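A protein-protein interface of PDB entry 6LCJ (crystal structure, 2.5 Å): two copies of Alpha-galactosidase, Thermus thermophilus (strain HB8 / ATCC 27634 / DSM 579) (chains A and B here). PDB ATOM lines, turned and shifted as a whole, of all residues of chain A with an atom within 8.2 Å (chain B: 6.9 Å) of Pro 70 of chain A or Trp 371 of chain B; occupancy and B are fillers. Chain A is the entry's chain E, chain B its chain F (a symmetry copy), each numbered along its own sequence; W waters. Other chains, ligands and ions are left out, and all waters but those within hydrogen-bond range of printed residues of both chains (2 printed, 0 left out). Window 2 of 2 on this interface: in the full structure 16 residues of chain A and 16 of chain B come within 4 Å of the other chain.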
ATOM      1  N   PRO A  67     -31.154 -28.839   8.827  1.00  0.00           N
ATOM      2  CA  PRO A  67     -30.196 -29.892   8.467  1.00  0.00           C
ATOM      3  C   PRO A  67     -28.951 -29.315   7.816  1.00  0.00           C
ATOM      4  O   PRO A  67     -29.020 -28.377   7.023  1.00  0.00           O
ATOM      5  CB  PRO A  67     -30.982 -30.772   7.489  1.00  0.00           C
ATOM      6  CG  PRO A  67     -32.437 -30.469   7.773  1.00  0.00           C
ATOM      7  CD  PRO A  67     -32.459 -29.026   8.171  1.00  0.00           C
ATOM      8  N   LEU A  68     -27.808 -29.897   8.155  1.00  0.00           N
ATOM      9  CA  LEU A  68     -26.518 -29.464   7.646  1.00  0.00           C
ATOM     10  C   LEU A  68     -26.202 -30.268   6.397  1.00  0.00           C
ATOM     11  O   LEU A  68     -26.341 -31.495   6.394  1.00  0.00           O
ATOM     12  CB  LEU A  68     -25.435 -29.666   8.710  1.00  0.00           C
ATOM     13  CG  LEU A  68     -24.017 -29.162   8.440  1.00  0.00           C
ATOM     14  CD1 LEU A  68     -23.367 -28.742   9.745  1.00  0.00           C
ATOM     15  CD2 LEU A  68     -23.163 -30.201   7.736  1.00  0.00           C
ATOM     16  N   LEU A  69     -25.774 -29.586   5.344  1.00  0.00           N
ATOM     17  CA  LEU A  69     -25.474 -30.207   4.065  1.00  0.00           C
ATOM     18  C   LEU A  69     -24.034 -29.924   3.687  1.00  0.00           C
ATOM     19  O   LEU A  69     -23.436 -28.955   4.171  1.00  0.00           O
ATOM     20  CB  LEU A  69     -26.406 -29.689   2.957  1.00  0.00           C
ATOM     21  CG  LEU A  69     -27.905 -29.919   3.175  1.00  0.00           C
ATOM     22  CD1 LEU A  69     -28.699 -29.429   1.982  1.00  0.00           C
ATOM     23  CD2 LEU A  69     -28.178 -31.379   3.456  1.00  0.00           C
ATOM     24  N   PRO A  70     -23.421 -30.778   2.851  1.00  0.00           N
ATOM     25  CA  PRO A  70     -23.953 -32.063   2.394  1.00  0.00           C
ATOM     26  C   PRO A  70     -23.859 -33.120   3.501  1.00  0.00           C
ATOM     27  O   PRO A  70     -23.102 -32.927   4.459  1.00  0.00           O
ATOM     28  CB  PRO A  70     -23.034 -32.407   1.237  1.00  0.00           C
ATOM     29  CG  PRO A  70     -21.733 -31.851   1.684  1.00  0.00           C
ATOM     30  CD  PRO A  70     -22.061 -30.550   2.334  1.00  0.00           C
ATOM     31  N   GLU A  71     -24.604 -34.219   3.368  1.00  0.00           N
ATOM     32  CA  GLU A  71     -24.523 -35.297   4.349  1.00  0.00           C
ATOM     33  C   GLU A  71     -23.081 -35.749   4.572  1.00  0.00           C
ATOM     34  O   GLU A  71     -22.682 -36.043   5.705  1.00  0.00           O
ATOM     35  CB  GLU A  71     -25.382 -36.472   3.886  1.00  0.00           C
ATOM     36  CG  GLU A  71     -26.198 -37.142   4.978  1.00  0.00           C
ATOM     37  CD  GLU A  71     -27.545 -37.647   4.473  1.00  0.00           C
ATOM     38  OE1 GLU A  71     -27.695 -38.875   4.271  1.00  0.00           O
ATOM     39  OE2 GLU A  71     -28.456 -36.814   4.283  1.00  0.00           O
ATOM     40  N   ALA A  72     -22.278 -35.792   3.502  1.00  0.00           N
ATOM     41  CA  ALA A  72     -20.926 -36.342   3.572  1.00  0.00           C
ATOM     42  C   ALA A  72     -20.024 -35.603   4.551  1.00  0.00           C
ATOM     43  O   ALA A  72     -19.010 -36.174   4.979  1.00  0.00           O
ATOM     44  CB  ALA A  72     -20.266 -36.313   2.192  1.00  0.00           C
ATOM     45  N   ARG A  73     -20.346 -34.340   4.885  1.00  0.00           N
ATOM     46  CA  ARG A  73     -19.523 -33.512   5.758  1.00  0.00           C
ATOM     47  C   ARG A  73     -19.989 -33.479   7.210  1.00  0.00           C
ATOM     48  O   ARG A  73     -19.317 -32.861   8.042  1.00  0.00           O
ATOM     49  CB  ARG A  73     -19.480 -32.089   5.231  1.00  0.00           C
ATOM     50  CG  ARG A  73     -18.449 -31.839   4.171  1.00  0.00           C
ATOM     51  CD  ARG A  73     -18.169 -30.363   4.169  1.00  0.00           C
ATOM     52  NE  ARG A  73     -17.366 -29.914   3.041  1.00  0.00           N
ATOM     53  CZ  ARG A  73     -17.703 -28.909   2.243  1.00  0.00           C
ATOM     54  NH1 ARG A  73     -18.846 -28.255   2.424  1.00  0.00           N
ATOM     55  NH2 ARG A  73     -16.897 -28.559   1.260  1.00  0.00           N
ATOM     56  N   ARG A  74     -21.115 -34.111   7.541  1.00  0.00           N
ATOM     57  CA  ARG A  74     -21.553 -34.147   8.934  1.00  0.00           C
ATOM     58  C   ARG A  74     -20.551 -34.769   9.904  1.00  0.00           C
ATOM     59  O   ARG A  74     -20.402 -34.226  11.011  1.00  0.00           O
ATOM     60  CB  ARG A  74     -22.894 -34.868   9.033  1.00  0.00           C
ATOM     61  CG  ARG A  74     -23.976 -34.088   8.378  1.00  0.00           C
ATOM     62  CD  ARG A  74     -25.267 -34.815   8.377  1.00  0.00           C
ATOM     63  NE  ARG A  74     -26.283 -33.946   7.809  1.00  0.00           N
ATOM     64  CZ  ARG A  74     -27.547 -34.296   7.614  1.00  0.00           C
ATOM     65  NH1 ARG A  74     -27.959 -35.510   7.955  1.00  0.00           N
ATOM     66  NH2 ARG A  74     -28.389 -33.431   7.074  1.00  0.00           N
ATOM     67  N   PRO A  75     -19.856 -35.868   9.594  1.00  0.00           N
ATOM     68  CA  PRO A  75     -18.924 -36.426  10.598  1.00  0.00           C
ATOM     69  C   PRO A  75     -17.793 -35.477  10.987  1.00  0.00           C
ATOM     70  O   PRO A  75     -17.240 -35.614  12.087  1.00  0.00           O
ATOM     71  CB  PRO A  75     -18.389 -37.699   9.923  1.00  0.00           C
ATOM     72  CG  PRO A  75     -19.449 -38.068   8.910  1.00  0.00           C
ATOM     73  CD  PRO A  75     -19.984 -36.746   8.413  1.00  0.00           C
ATOM     74  N   GLN A  76     -17.436 -34.510  10.144  1.00  0.00           N
ATOM     75  CA  GLN A  76     -16.385 -33.558  10.480  1.00  0.00           C
ATOM     76  C   GLN A  76     -16.931 -32.210  10.944  1.00  0.00           C
ATOM     77  O   GLN A  76     -16.145 -31.290  11.177  1.00  0.00           O
ATOM     78  CB  GLN A  76     -15.438 -33.355   9.290  1.00  0.00           C
ATOM     79  CG  GLN A  76     -15.890 -32.319   8.284  1.00  0.00           C
ATOM     80  CD  GLN A  76     -15.533 -32.725   6.865  1.00  0.00           C
ATOM     81  OE1 GLN A  76     -15.558 -33.907   6.541  1.00  0.00           O
ATOM     82  NE2 GLN A  76     -15.206 -31.751   6.009  1.00  0.00           N
ATOM     83  N   ALA A  77     -18.252 -32.079  11.089  1.00  0.00           N
ATOM     84  CA  ALA A  77     -18.903 -30.860  11.545  1.00  0.00           C
ATOM     85  C   ALA A  77     -19.279 -30.910  13.023  1.00  0.00           C
ATOM     86  O   ALA A  77     -19.126 -29.911  13.735  1.00  0.00           O
ATOM     87  CB  ALA A  77     -20.156 -30.582  10.703  1.00  0.00           C
ATOM     88  N   LEU A  83     -26.591 -33.790  14.851  1.00  0.00           N
ATOM     89  CA  LEU A  83     -26.920 -33.262  13.538  1.00  0.00           C
ATOM     90  C   LEU A  83     -28.040 -34.031  12.846  1.00  0.00           C
ATOM     91  O   LEU A  83     -28.586 -33.536  11.859  1.00  0.00           O
ATOM     92  CB  LEU A  83     -25.672 -33.264  12.643  1.00  0.00           C
ATOM     93  CG  LEU A  83     -24.531 -32.332  13.046  1.00  0.00           C
ATOM     94  CD1 LEU A  83     -23.429 -32.373  12.016  1.00  0.00           C
ATOM     95  CD2 LEU A  83     -25.029 -30.908  13.252  1.00  0.00           C
ATOM     96  N   GLU A  84     -28.382 -35.230  13.316  1.00  0.00           N
ATOM     97  CA  GLU A  84     -29.492 -35.981  12.750  1.00  0.00           C
ATOM     98  C   GLU A  84     -30.789 -35.793  13.526  1.00  0.00           C
ATOM     99  O   GLU A  84     -31.824 -36.308  13.095  1.00  0.00           O
ATOM    100  CB  GLU A  84     -29.168 -37.492  12.685  1.00  0.00           C
ATOM    101  CG  GLU A  84     -27.813 -37.865  12.073  1.00  0.00           C
ATOM    102  CD  GLU A  84     -27.764 -37.753  10.545  1.00  0.00           C
ATOM    103  OE1 GLU A  84     -28.804 -38.012   9.891  1.00  0.00           O
ATOM    104  OE2 GLU A  84     -26.687 -37.402  10.006  1.00  0.00           O
ATOM    105  N   GLY A 265     -15.959 -38.092   7.084  1.00  0.00           N
ATOM    106  CA  GLY A 265     -16.123 -36.827   6.404  1.00  0.00           C
ATOM    107  C   GLY A 265     -15.561 -36.755   4.999  1.00  0.00           C
ATOM    108  O   GLY A 265     -15.283 -37.777   4.367  1.00  0.00           O
ATOM    109  N   PHE A 266     -15.388 -35.535   4.501  1.00  0.00           N
ATOM    110  CA  PHE A 266     -14.973 -35.300   3.125  1.00  0.00           C
ATOM    111  C   PHE A 266     -14.065 -34.083   3.092  1.00  0.00           C
ATOM    112  O   PHE A 266     -14.492 -32.976   3.432  1.00  0.00           O
ATOM    113  CB  PHE A 266     -16.183 -35.092   2.221  1.00  0.00           C
ATOM    114  CG  PHE A 266     -15.862 -35.170   0.768  1.00  0.00           C
ATOM    115  CD1 PHE A 266     -15.411 -34.049   0.079  1.00  0.00           C
ATOM    116  CD2 PHE A 266     -15.994 -36.370   0.082  1.00  0.00           C
ATOM    117  CE1 PHE A 266     -15.110 -34.128  -1.267  1.00  0.00           C
ATOM    118  CE2 PHE A 266     -15.685 -36.459  -1.268  1.00  0.00           C
ATOM    119  CZ  PHE A 266     -15.250 -35.339  -1.945  1.00  0.00           C
ATOM    120  N   ASN A 267     -12.823 -34.287   2.673  1.00  0.00           N
ATOM    121  CA  ASN A 267     -11.828 -33.225   2.674  1.00  0.00           C
ATOM    122  C   ASN A 267     -10.731 -33.614   1.699  1.00  0.00           C
ATOM    123  O   ASN A 267     -10.588 -34.787   1.344  1.00  0.00           O
ATOM    124  CB  ASN A 267     -11.265 -32.985   4.080  1.00  0.00           C
ATOM    125  CG  ASN A 267     -10.691 -31.590   4.249  1.00  0.00           C
ATOM    126  OD1 ASN A 267     -11.227 -30.617   3.722  1.00  0.00           O
ATOM    127  ND2 ASN A 267      -9.592 -31.489   4.990  1.00  0.00           N
ATOM    128  N   GLY A 269     -10.825 -33.280  -1.279  1.00  0.00           N
ATOM    129  CA  GLY A 269     -11.477 -33.890  -2.425  1.00  0.00           C
ATOM    130  C   GLY A 269     -11.814 -35.363  -2.327  1.00  0.00           C
ATOM    131  O   GLY A 269     -12.212 -35.951  -3.339  1.00  0.00           O
ATOM    132  N   ARG A 270     -11.706 -35.984  -1.159  1.00  0.00           N
ATOM    133  CA  ARG A 270     -11.945 -37.417  -1.054  1.00  0.00           C
ATOM    134  C   ARG A 270     -12.639 -37.780   0.251  1.00  0.00           C
ATOM    135  O   ARG A 270     -12.545 -37.049   1.246  1.00  0.00           O
ATOM    136  CB  ARG A 270     -10.628 -38.195  -1.166  1.00  0.00           C
ATOM    137  CG  ARG A 270      -9.527 -37.595  -0.345  1.00  0.00           C
ATOM    138  CD  ARG A 270      -8.246 -38.318  -0.631  1.00  0.00           C
ATOM    139  NE  ARG A 270      -8.101 -38.585  -2.051  1.00  0.00           N
ATOM    140  CZ  ARG A 270      -7.141 -38.056  -2.798  1.00  0.00           C
ATOM    141  NH1 ARG A 270      -6.256 -37.234  -2.239  1.00  0.00           N
ATOM    142  NH2 ARG A 270      -7.066 -38.344  -4.093  1.00  0.00           N
ATOM    143  N   GLU A 367     -22.458 -19.351   0.497  1.00  0.00           N
ATOM    144  CA  GLU A 367     -22.939 -20.601  -0.082  1.00  0.00           C
ATOM    145  C   GLU A 367     -22.856 -21.741   0.924  1.00  0.00           C
ATOM    146  O   GLU A 367     -23.778 -22.554   1.030  1.00  0.00           O
ATOM    147  CB  GLU A 367     -22.160 -20.947  -1.348  1.00  0.00           C
ATOM    148  CG  GLU A 367     -22.853 -20.435  -2.602  1.00  0.00           C
ATOM    149  CD  GLU A 367     -22.828 -18.936  -2.637  1.00  0.00           C
ATOM    150  OE1 GLU A 367     -21.724 -18.399  -2.450  1.00  0.00           O
ATOM    151  OE2 GLU A 367     -23.888 -18.298  -2.805  1.00  0.00           O
ATOM    152  N   ARG A 368     -21.768 -21.810   1.689  1.00  0.00           N
ATOM    153  CA  ARG A 368     -21.641 -22.881   2.672  1.00  0.00           C
ATOM    154  C   ARG A 368     -22.377 -22.557   3.971  1.00  0.00           C
ATOM    155  O   ARG A 368     -23.013 -23.437   4.565  1.00  0.00           O
ATOM    156  CB  ARG A 368     -20.166 -23.172   2.940  1.00  0.00           C
ATOM    157  CG  ARG A 368     -19.947 -24.239   3.984  1.00  0.00           C
ATOM    158  CD  ARG A 368     -18.527 -24.780   3.934  1.00  0.00           C
ATOM    159  NE  ARG A 368     -18.364 -25.850   4.903  1.00  0.00           N
ATOM    160  CZ  ARG A 368     -17.234 -26.510   5.130  1.00  0.00           C
ATOM    161  NH1 ARG A 368     -16.131 -26.228   4.447  1.00  0.00           N
ATOM    162  NH2 ARG A 368     -17.219 -27.457   6.050  1.00  0.00           N
ATOM    163  N   TRP A 371     -26.675 -21.581   2.290  1.00  0.00           N
ATOM    164  CA  TRP A 371     -27.359 -22.525   1.413  1.00  0.00           C
ATOM    165  C   TRP A 371     -27.159 -23.965   1.866  1.00  0.00           C
ATOM    166  O   TRP A 371     -28.089 -24.778   1.797  1.00  0.00           O
ATOM    167  CB  TRP A 371     -26.892 -22.323  -0.026  1.00  0.00           C
ATOM    168  CG  TRP A 371     -27.330 -20.987  -0.531  1.00  0.00           C
ATOM    169  CD1 TRP A 371     -26.544 -19.906  -0.756  1.00  0.00           C
ATOM    170  CD2 TRP A 371     -28.674 -20.583  -0.835  1.00  0.00           C
ATOM    171  NE1 TRP A 371     -27.304 -18.848  -1.200  1.00  0.00           N
ATOM    172  CE2 TRP A 371     -28.617 -19.237  -1.257  1.00  0.00           C
ATOM    173  CE3 TRP A 371     -29.919 -21.232  -0.801  1.00  0.00           C
ATOM    174  CZ2 TRP A 371     -29.762 -18.519  -1.651  1.00  0.00           C
ATOM    175  CZ3 TRP A 371     -31.060 -20.515  -1.192  1.00  0.00           C
ATOM    176  CH2 TRP A 371     -30.967 -19.172  -1.607  1.00  0.00           C
ATOM    177  N   LEU A 372     -25.973 -24.298   2.354  1.00  0.00           N
ATOM    178  CA  LEU A 372     -25.737 -25.621   2.908  1.00  0.00           C
ATOM    179  C   LEU A 372     -25.938 -25.668   4.419  1.00  0.00           C
ATOM    180  O   LEU A 372     -25.829 -26.746   5.014  1.00  0.00           O
ATOM    181  CB  LEU A 372     -24.325 -26.090   2.532  1.00  0.00           C
ATOM    182  CG  LEU A 372     -24.071 -26.118   1.021  1.00  0.00           C
ATOM    183  CD1 LEU A 372     -22.585 -26.222   0.719  1.00  0.00           C
ATOM    184  CD2 LEU A 372     -24.829 -27.253   0.375  1.00  0.00           C
ATOM    185  N   ALA A 373     -26.212 -24.528   5.050  1.00  0.00           N
ATOM    186  CA  ALA A 373     -26.497 -24.453   6.482  1.00  0.00           C
ATOM    187  C   ALA A 373     -25.385 -25.114   7.308  1.00  0.00           C
ATOM    188  O   ALA A 373     -25.634 -25.925   8.206  1.00  0.00           O
ATOM    189  CB  ALA A 373     -27.865 -25.068   6.781  1.00  0.00           C
ATOM    190  N   ASP A 374     -24.135 -24.764   6.984  1.00  0.00           N
ATOM    191  CA  ASP A 374     -22.943 -25.326   7.628  1.00  0.00           C
ATOM    192  C   ASP A 374     -22.140 -24.201   8.268  1.00  0.00           C
ATOM    193  O   ASP A 374     -21.244 -23.620   7.632  1.00  0.00           O
ATOM    194  CB  ASP A 374     -22.087 -26.100   6.627  1.00  0.00           C
ATOM    195  CG  ASP A 374     -20.807 -26.659   7.247  1.00  0.00           C
ATOM    196  OD1 ASP A 374     -20.641 -26.621   8.494  1.00  0.00           O
ATOM    197  OD2 ASP A 374     -19.955 -27.151   6.475  1.00  0.00           O
ATOM    198  N   PRO B  67     -28.141 -31.405 -11.671  1.00  0.00           N
ATOM    199  CA  PRO B  67     -29.032 -30.284 -11.333  1.00  0.00           C
ATOM    200  C   PRO B  67     -28.287 -29.142 -10.653  1.00  0.00           C
ATOM    201  O   PRO B  67     -27.380 -29.361  -9.845  1.00  0.00           O
ATOM    202  CB  PRO B  67     -30.056 -30.925 -10.389  1.00  0.00           C
ATOM    203  CG  PRO B  67     -29.996 -32.425 -10.710  1.00  0.00           C
ATOM    204  CD  PRO B  67     -28.584 -32.687 -11.090  1.00  0.00           C
ATOM    205  N   LEU B  69     -28.158 -26.094  -8.033  1.00  0.00           N
ATOM    206  CA  LEU B  69     -28.816 -25.717  -6.789  1.00  0.00           C
ATOM    207  C   LEU B  69     -28.303 -24.360  -6.320  1.00  0.00           C
ATOM    208  O   LEU B  69     -27.179 -23.971  -6.659  1.00  0.00           O
ATOM    209  CB  LEU B  69     -28.591 -26.761  -5.684  1.00  0.00           C
ATOM    210  CG  LEU B  69     -28.909 -28.216  -6.057  1.00  0.00           C
ATOM    211  CD1 LEU B  69     -28.321 -29.187  -5.044  1.00  0.00           C
ATOM    212  CD2 LEU B  69     -30.406 -28.406  -6.178  1.00  0.00           C
ATOM    213  N   ASN B 365     -15.220 -20.638  -5.953  1.00  0.00           N
ATOM    214  CA  ASN B 365     -15.957 -20.950  -4.736  1.00  0.00           C
ATOM    215  C   ASN B 365     -16.462 -22.384  -4.893  1.00  0.00           C
ATOM    216  O   ASN B 365     -17.485 -22.633  -5.538  1.00  0.00           O
ATOM    217  CB  ASN B 365     -17.084 -19.949  -4.521  1.00  0.00           C
ATOM    218  CG  ASN B 365     -17.829 -20.170  -3.220  1.00  0.00           C
ATOM    219  OD1 ASN B 365     -17.765 -21.239  -2.630  1.00  0.00           O
ATOM    220  ND2 ASN B 365     -18.555 -19.152  -2.773  1.00  0.00           N
ATOM    221  N   GLU B 366     -15.724 -23.329  -4.301  1.00  0.00           N
ATOM    222  CA  GLU B 366     -16.011 -24.749  -4.457  1.00  0.00           C
ATOM    223  C   GLU B 366     -17.396 -25.119  -3.939  1.00  0.00           C
ATOM    224  O   GLU B 366     -18.038 -26.036  -4.472  1.00  0.00           O
ATOM    225  CB  GLU B 366     -14.949 -25.555  -3.718  1.00  0.00           C
ATOM    226  CG  GLU B 366     -14.032 -26.372  -4.593  1.00  0.00           C
ATOM    227  CD  GLU B 366     -12.842 -26.945  -3.812  1.00  0.00           C
ATOM    228  OE1 GLU B 366     -12.924 -28.123  -3.384  1.00  0.00           O
ATOM    229  OE2 GLU B 366     -11.830 -26.224  -3.630  1.00  0.00           O
ATOM    230  N   GLU B 367     -17.853 -24.447  -2.881  1.00  0.00           N
ATOM    231  CA  GLU B 367     -19.169 -24.728  -2.322  1.00  0.00           C
ATOM    232  C   GLU B 367     -20.269 -24.439  -3.331  1.00  0.00           C
ATOM    233  O   GLU B 367     -21.273 -25.160  -3.396  1.00  0.00           O
ATOM    234  CB  GLU B 367     -19.375 -23.903  -1.055  1.00  0.00           C
ATOM    235  CG  GLU B 367     -18.164 -23.940  -0.135  1.00  0.00           C
ATOM    236  CD  GLU B 367     -17.883 -25.336   0.378  1.00  0.00           C
ATOM    237  OE1 GLU B 367     -18.846 -26.048   0.740  1.00  0.00           O
ATOM    238  OE2 GLU B 367     -16.703 -25.738   0.401  1.00  0.00           O
ATOM    239  N   ARG B 368     -20.092 -23.400  -4.142  1.00  0.00           N
ATOM    240  CA  ARG B 368     -21.075 -23.115  -5.178  1.00  0.00           C
ATOM    241  C   ARG B 368     -20.819 -23.895  -6.476  1.00  0.00           C
ATOM    242  O   ARG B 368     -21.765 -24.356  -7.116  1.00  0.00           O
ATOM    243  CB  ARG B 368     -21.113 -21.605  -5.445  1.00  0.00           C
ATOM    244  CG  ARG B 368     -22.235 -21.200  -6.365  1.00  0.00           C
ATOM    245  CD  ARG B 368     -22.410 -19.722  -6.422  1.00  0.00           C
ATOM    246  NE  ARG B 368     -23.451 -19.370  -7.372  1.00  0.00           N
ATOM    247  CZ  ARG B 368     -23.974 -18.152  -7.500  1.00  0.00           C
ATOM    248  NH1 ARG B 368     -23.545 -17.154  -6.729  1.00  0.00           N
ATOM    249  NH2 ARG B 368     -24.934 -17.943  -8.396  1.00  0.00           N
ATOM    250  N   SER B 369     -19.566 -24.071  -6.886  1.00  0.00           N
ATOM    251  CA  SER B 369     -19.294 -24.729  -8.164  1.00  0.00           C
ATOM    252  C   SER B 369     -19.515 -26.231  -8.087  1.00  0.00           C
ATOM    253  O   SER B 369     -19.999 -26.841  -9.045  1.00  0.00           O
ATOM    254  CB  SER B 369     -17.865 -24.440  -8.616  1.00  0.00           C
ATOM    255  OG  SER B 369     -17.697 -23.047  -8.824  1.00  0.00           O
ATOM    256  N   PHE B 370     -19.169 -26.842  -6.959  1.00  0.00           N
ATOM    257  CA  PHE B 370     -19.206 -28.282  -6.828  1.00  0.00           C
ATOM    258  C   PHE B 370     -20.434 -28.738  -6.041  1.00  0.00           C
ATOM    259  O   PHE B 370     -21.332 -29.363  -6.607  1.00  0.00           O
ATOM    260  CB  PHE B 370     -17.912 -28.762  -6.170  1.00  0.00           C
ATOM    261  CG  PHE B 370     -17.869 -30.238  -5.952  1.00  0.00           C
ATOM    262  CD1 PHE B 370     -17.574 -31.095  -6.993  1.00  0.00           C
ATOM    263  CD2 PHE B 370     -18.151 -30.772  -4.703  1.00  0.00           C
ATOM    264  CE1 PHE B 370     -17.551 -32.464  -6.788  1.00  0.00           C
ATOM    265  CE2 PHE B 370     -18.136 -32.130  -4.490  1.00  0.00           C
ATOM    266  CZ  PHE B 370     -17.830 -32.979  -5.535  1.00  0.00           C
ATOM    267  N   TRP B 371     -20.505 -28.409  -4.746  1.00  0.00           N
ATOM    268  CA  TRP B 371     -21.596 -28.908  -3.907  1.00  0.00           C
ATOM    269  C   TRP B 371     -22.964 -28.442  -4.402  1.00  0.00           C
ATOM    270  O   TRP B 371     -23.931 -29.211  -4.369  1.00  0.00           O
ATOM    271  CB  TRP B 371     -21.363 -28.492  -2.455  1.00  0.00           C
ATOM    272  CG  TRP B 371     -20.179 -29.221  -1.869  1.00  0.00           C
ATOM    273  CD1 TRP B 371     -18.965 -28.693  -1.558  1.00  0.00           C
ATOM    274  CD2 TRP B 371     -20.088 -30.625  -1.582  1.00  0.00           C
ATOM    275  NE1 TRP B 371     -18.128 -29.669  -1.089  1.00  0.00           N
ATOM    276  CE2 TRP B 371     -18.796 -30.863  -1.083  1.00  0.00           C
ATOM    277  CE3 TRP B 371     -20.973 -31.699  -1.702  1.00  0.00           C
ATOM    278  CZ2 TRP B 371     -18.365 -32.133  -0.698  1.00  0.00           C
ATOM    279  CZ3 TRP B 371     -20.540 -32.960  -1.321  1.00  0.00           C
ATOM    280  CH2 TRP B 371     -19.253 -33.163  -0.826  1.00  0.00           C
ATOM    281  N   LEU B 372     -23.075 -27.199  -4.880  1.00  0.00           N
ATOM    282  CA  LEU B 372     -24.331 -26.728  -5.467  1.00  0.00           C
ATOM    283  C   LEU B 372     -24.368 -26.851  -6.983  1.00  0.00           C
ATOM    284  O   LEU B 372     -25.375 -26.478  -7.590  1.00  0.00           O
ATOM    285  CB  LEU B 372     -24.609 -25.280  -5.084  1.00  0.00           C
ATOM    286  CG  LEU B 372     -24.651 -24.966  -3.601  1.00  0.00           C
ATOM    287  CD1 LEU B 372     -24.688 -23.460  -3.442  1.00  0.00           C
ATOM    288  CD2 LEU B 372     -25.868 -25.615  -2.970  1.00  0.00           C
ATOM    289  N   ALA B 373     -23.301 -27.358  -7.602  1.00  0.00           N
ATOM    290  CA  ALA B 373     -23.266 -27.613  -9.042  1.00  0.00           C
ATOM    291  C   ALA B 373     -23.709 -26.383  -9.844  1.00  0.00           C
ATOM    292  O   ALA B 373     -24.418 -26.485 -10.854  1.00  0.00           O
ATOM    293  CB  ALA B 373     -24.109 -28.839  -9.394  1.00  0.00           C
ATOM    294  N   ASP B 374     -23.285 -25.197  -9.393  1.00  0.00           N
ATOM    295  CA  ASP B 374     -23.589 -23.961 -10.107  1.00  0.00           C
ATOM    296  C   ASP B 374     -22.321 -23.367 -10.714  1.00  0.00           C
ATOM    297  O   ASP B 374     -21.566 -22.677 -10.019  1.00  0.00           O
ATOM    298  CB  ASP B 374     -24.267 -22.945  -9.184  1.00  0.00           C
ATOM    299  CG  ASP B 374     -24.563 -21.618  -9.899  1.00  0.00           C
ATOM    300  OD1 ASP B 374     -24.495 -21.595 -11.152  1.00  0.00           O
ATOM    301  OD2 ASP B 374     -24.844 -20.602  -9.217  1.00  0.00           O
HETATM  302  O   HOH W   1     -21.815 -16.566  -4.734  1.00  0.00           O
HETATM  303  O   HOH W   2     -15.223 -24.508   2.453  1.00  0.00           O
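The guanidinium group of Arg 73 of chain A lies within salt-bridge range of the side-chain carboxylate of Glu 367 of chain B (2.8 Å). The side-chain carboxylate (OE1) of Glu 367 of chain A is in hydrogen-bond range of the side-chain amide nitrogen (ND2) of Asn 365 of chain B (3.3 Å). NH2 of Arg 73 of chain A lies close to NE1 of Trp 371 of chain B, at 2.9 Å.
The guanidinium group (NE) of Arg 368 of chain A lies within salt-bridge range of the side-chain carboxylate (OD2) of Asp 374 of chain A, 2.6 Å away. OD1 of Asn 365 of chain B sits close to N of Glu 367 of chain B. The backbone carbonyl oxygen (O) of Glu 366 of chain B sits at hydrogen-bond distance from the backbone NH (N) of Trp 371 of chain B (3.4 Å). The guanidinium group (NE) of Arg 368 of chain B lies within salt-bridge range of the side-chain carboxylate (OD2) of Asp 374 of chain B, 2.6 Å away.
Among the printed residues, merely in contact across the chains: Pro 70 of chain A with Trp 371 of chain B (3.4 Å), Arg 368 of chain A with Glu 367 of chain B (3.5 Å), Glu 367 of chain A with Arg 368 of chain B (3.5 Å), Phe 266 of chain A with Trp 371 of chain B (3.6 Å), Glu 367 of chain A with Leu 372 of chain B (3.6 Å), Leu 372 of chain A with Glu 367 of chain B (3.7 Å) and Leu 372 of chain A with Leu 372 of chain B (3.9 Å).
Of chain B, only Trp 371 comes within 4 Å of Pro 70 of chain A. Of chain A, only Pro 70, Arg 73 and Phe 266 come within 4 Å of Trp 371 of chain B. Printed residues of chain A within 4 Å of Glu 367 of chain B: Arg 73 (2.8 Å), Arg 368 (3.5 Å) and Leu 372 (3.7 Å). Printed residues of chain B within 4 Å of Leu 372 of chain A: Glu 367 and Leu 372. Printed residues of chain A within 4 Å of Asn 365 of chain B: Glu 367 (3.3 Å). Glu 71 of chain A touches none of the printed residues of chain B. Leu 69 of chain A touches none of the printed residues of chain B. The nearest residue of chain B that does not touch Pro 70 of chain A is Glu 367 of chain B (5.8 Å). The nearest printed residue of chain B that does not touch Leu 372 of chain A is Trp 371 of chain B (4.1 Å).
Of the 24 printed residues of chain A, 6 touch a printed residue of chain B. Printed residues of chain A that touch a printed residue of chain B: Pro 70, Arg 73, Phe 266, Glu 367, Arg 368 and Leu 372. Of the 12 printed residues of chain B, 5 touch a printed residue of chain A. Along chain B the printed residues that touch a printed residue of chain A span positions 365 to 372. Among the printed residues, Asp or Glu carboxylates within 4 Å of a Lys or Arg side-chain nitrogen of the other chain: Arg 73 of chain A with Glu 367 of chain B (2.8 Å).
Glu 367 of chain A touches Arg 368 of chain B, and with the chains exchanged Arg 368 of chain A touches Glu 367 of chain B. Glu 367 of chain A touches Leu 372 of chain B, and with the chains exchanged Leu 372 of chain A touches Glu 367 of chain B. Leu 372 of chain B touches its own counterpart, Leu 372 of chain A. Positions printed for both chains: 67, 69, 367, 368, 371, 372, 373 and 374. Of the 10 pairs that touch across the chains among the printed residues, 5 have their exchanged pair printed and touching as well.
Water W1 bridges NH1 of Arg 368 of chain B (2.7 Å) and OE1 of Glu 367 of chain A (2.9 Å). Water W2 lies within hydrogen-bond range of NH1 of Arg 368 of chain A (2.8 Å) and OE2 of Glu 367 of chain B (2.8 Å).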
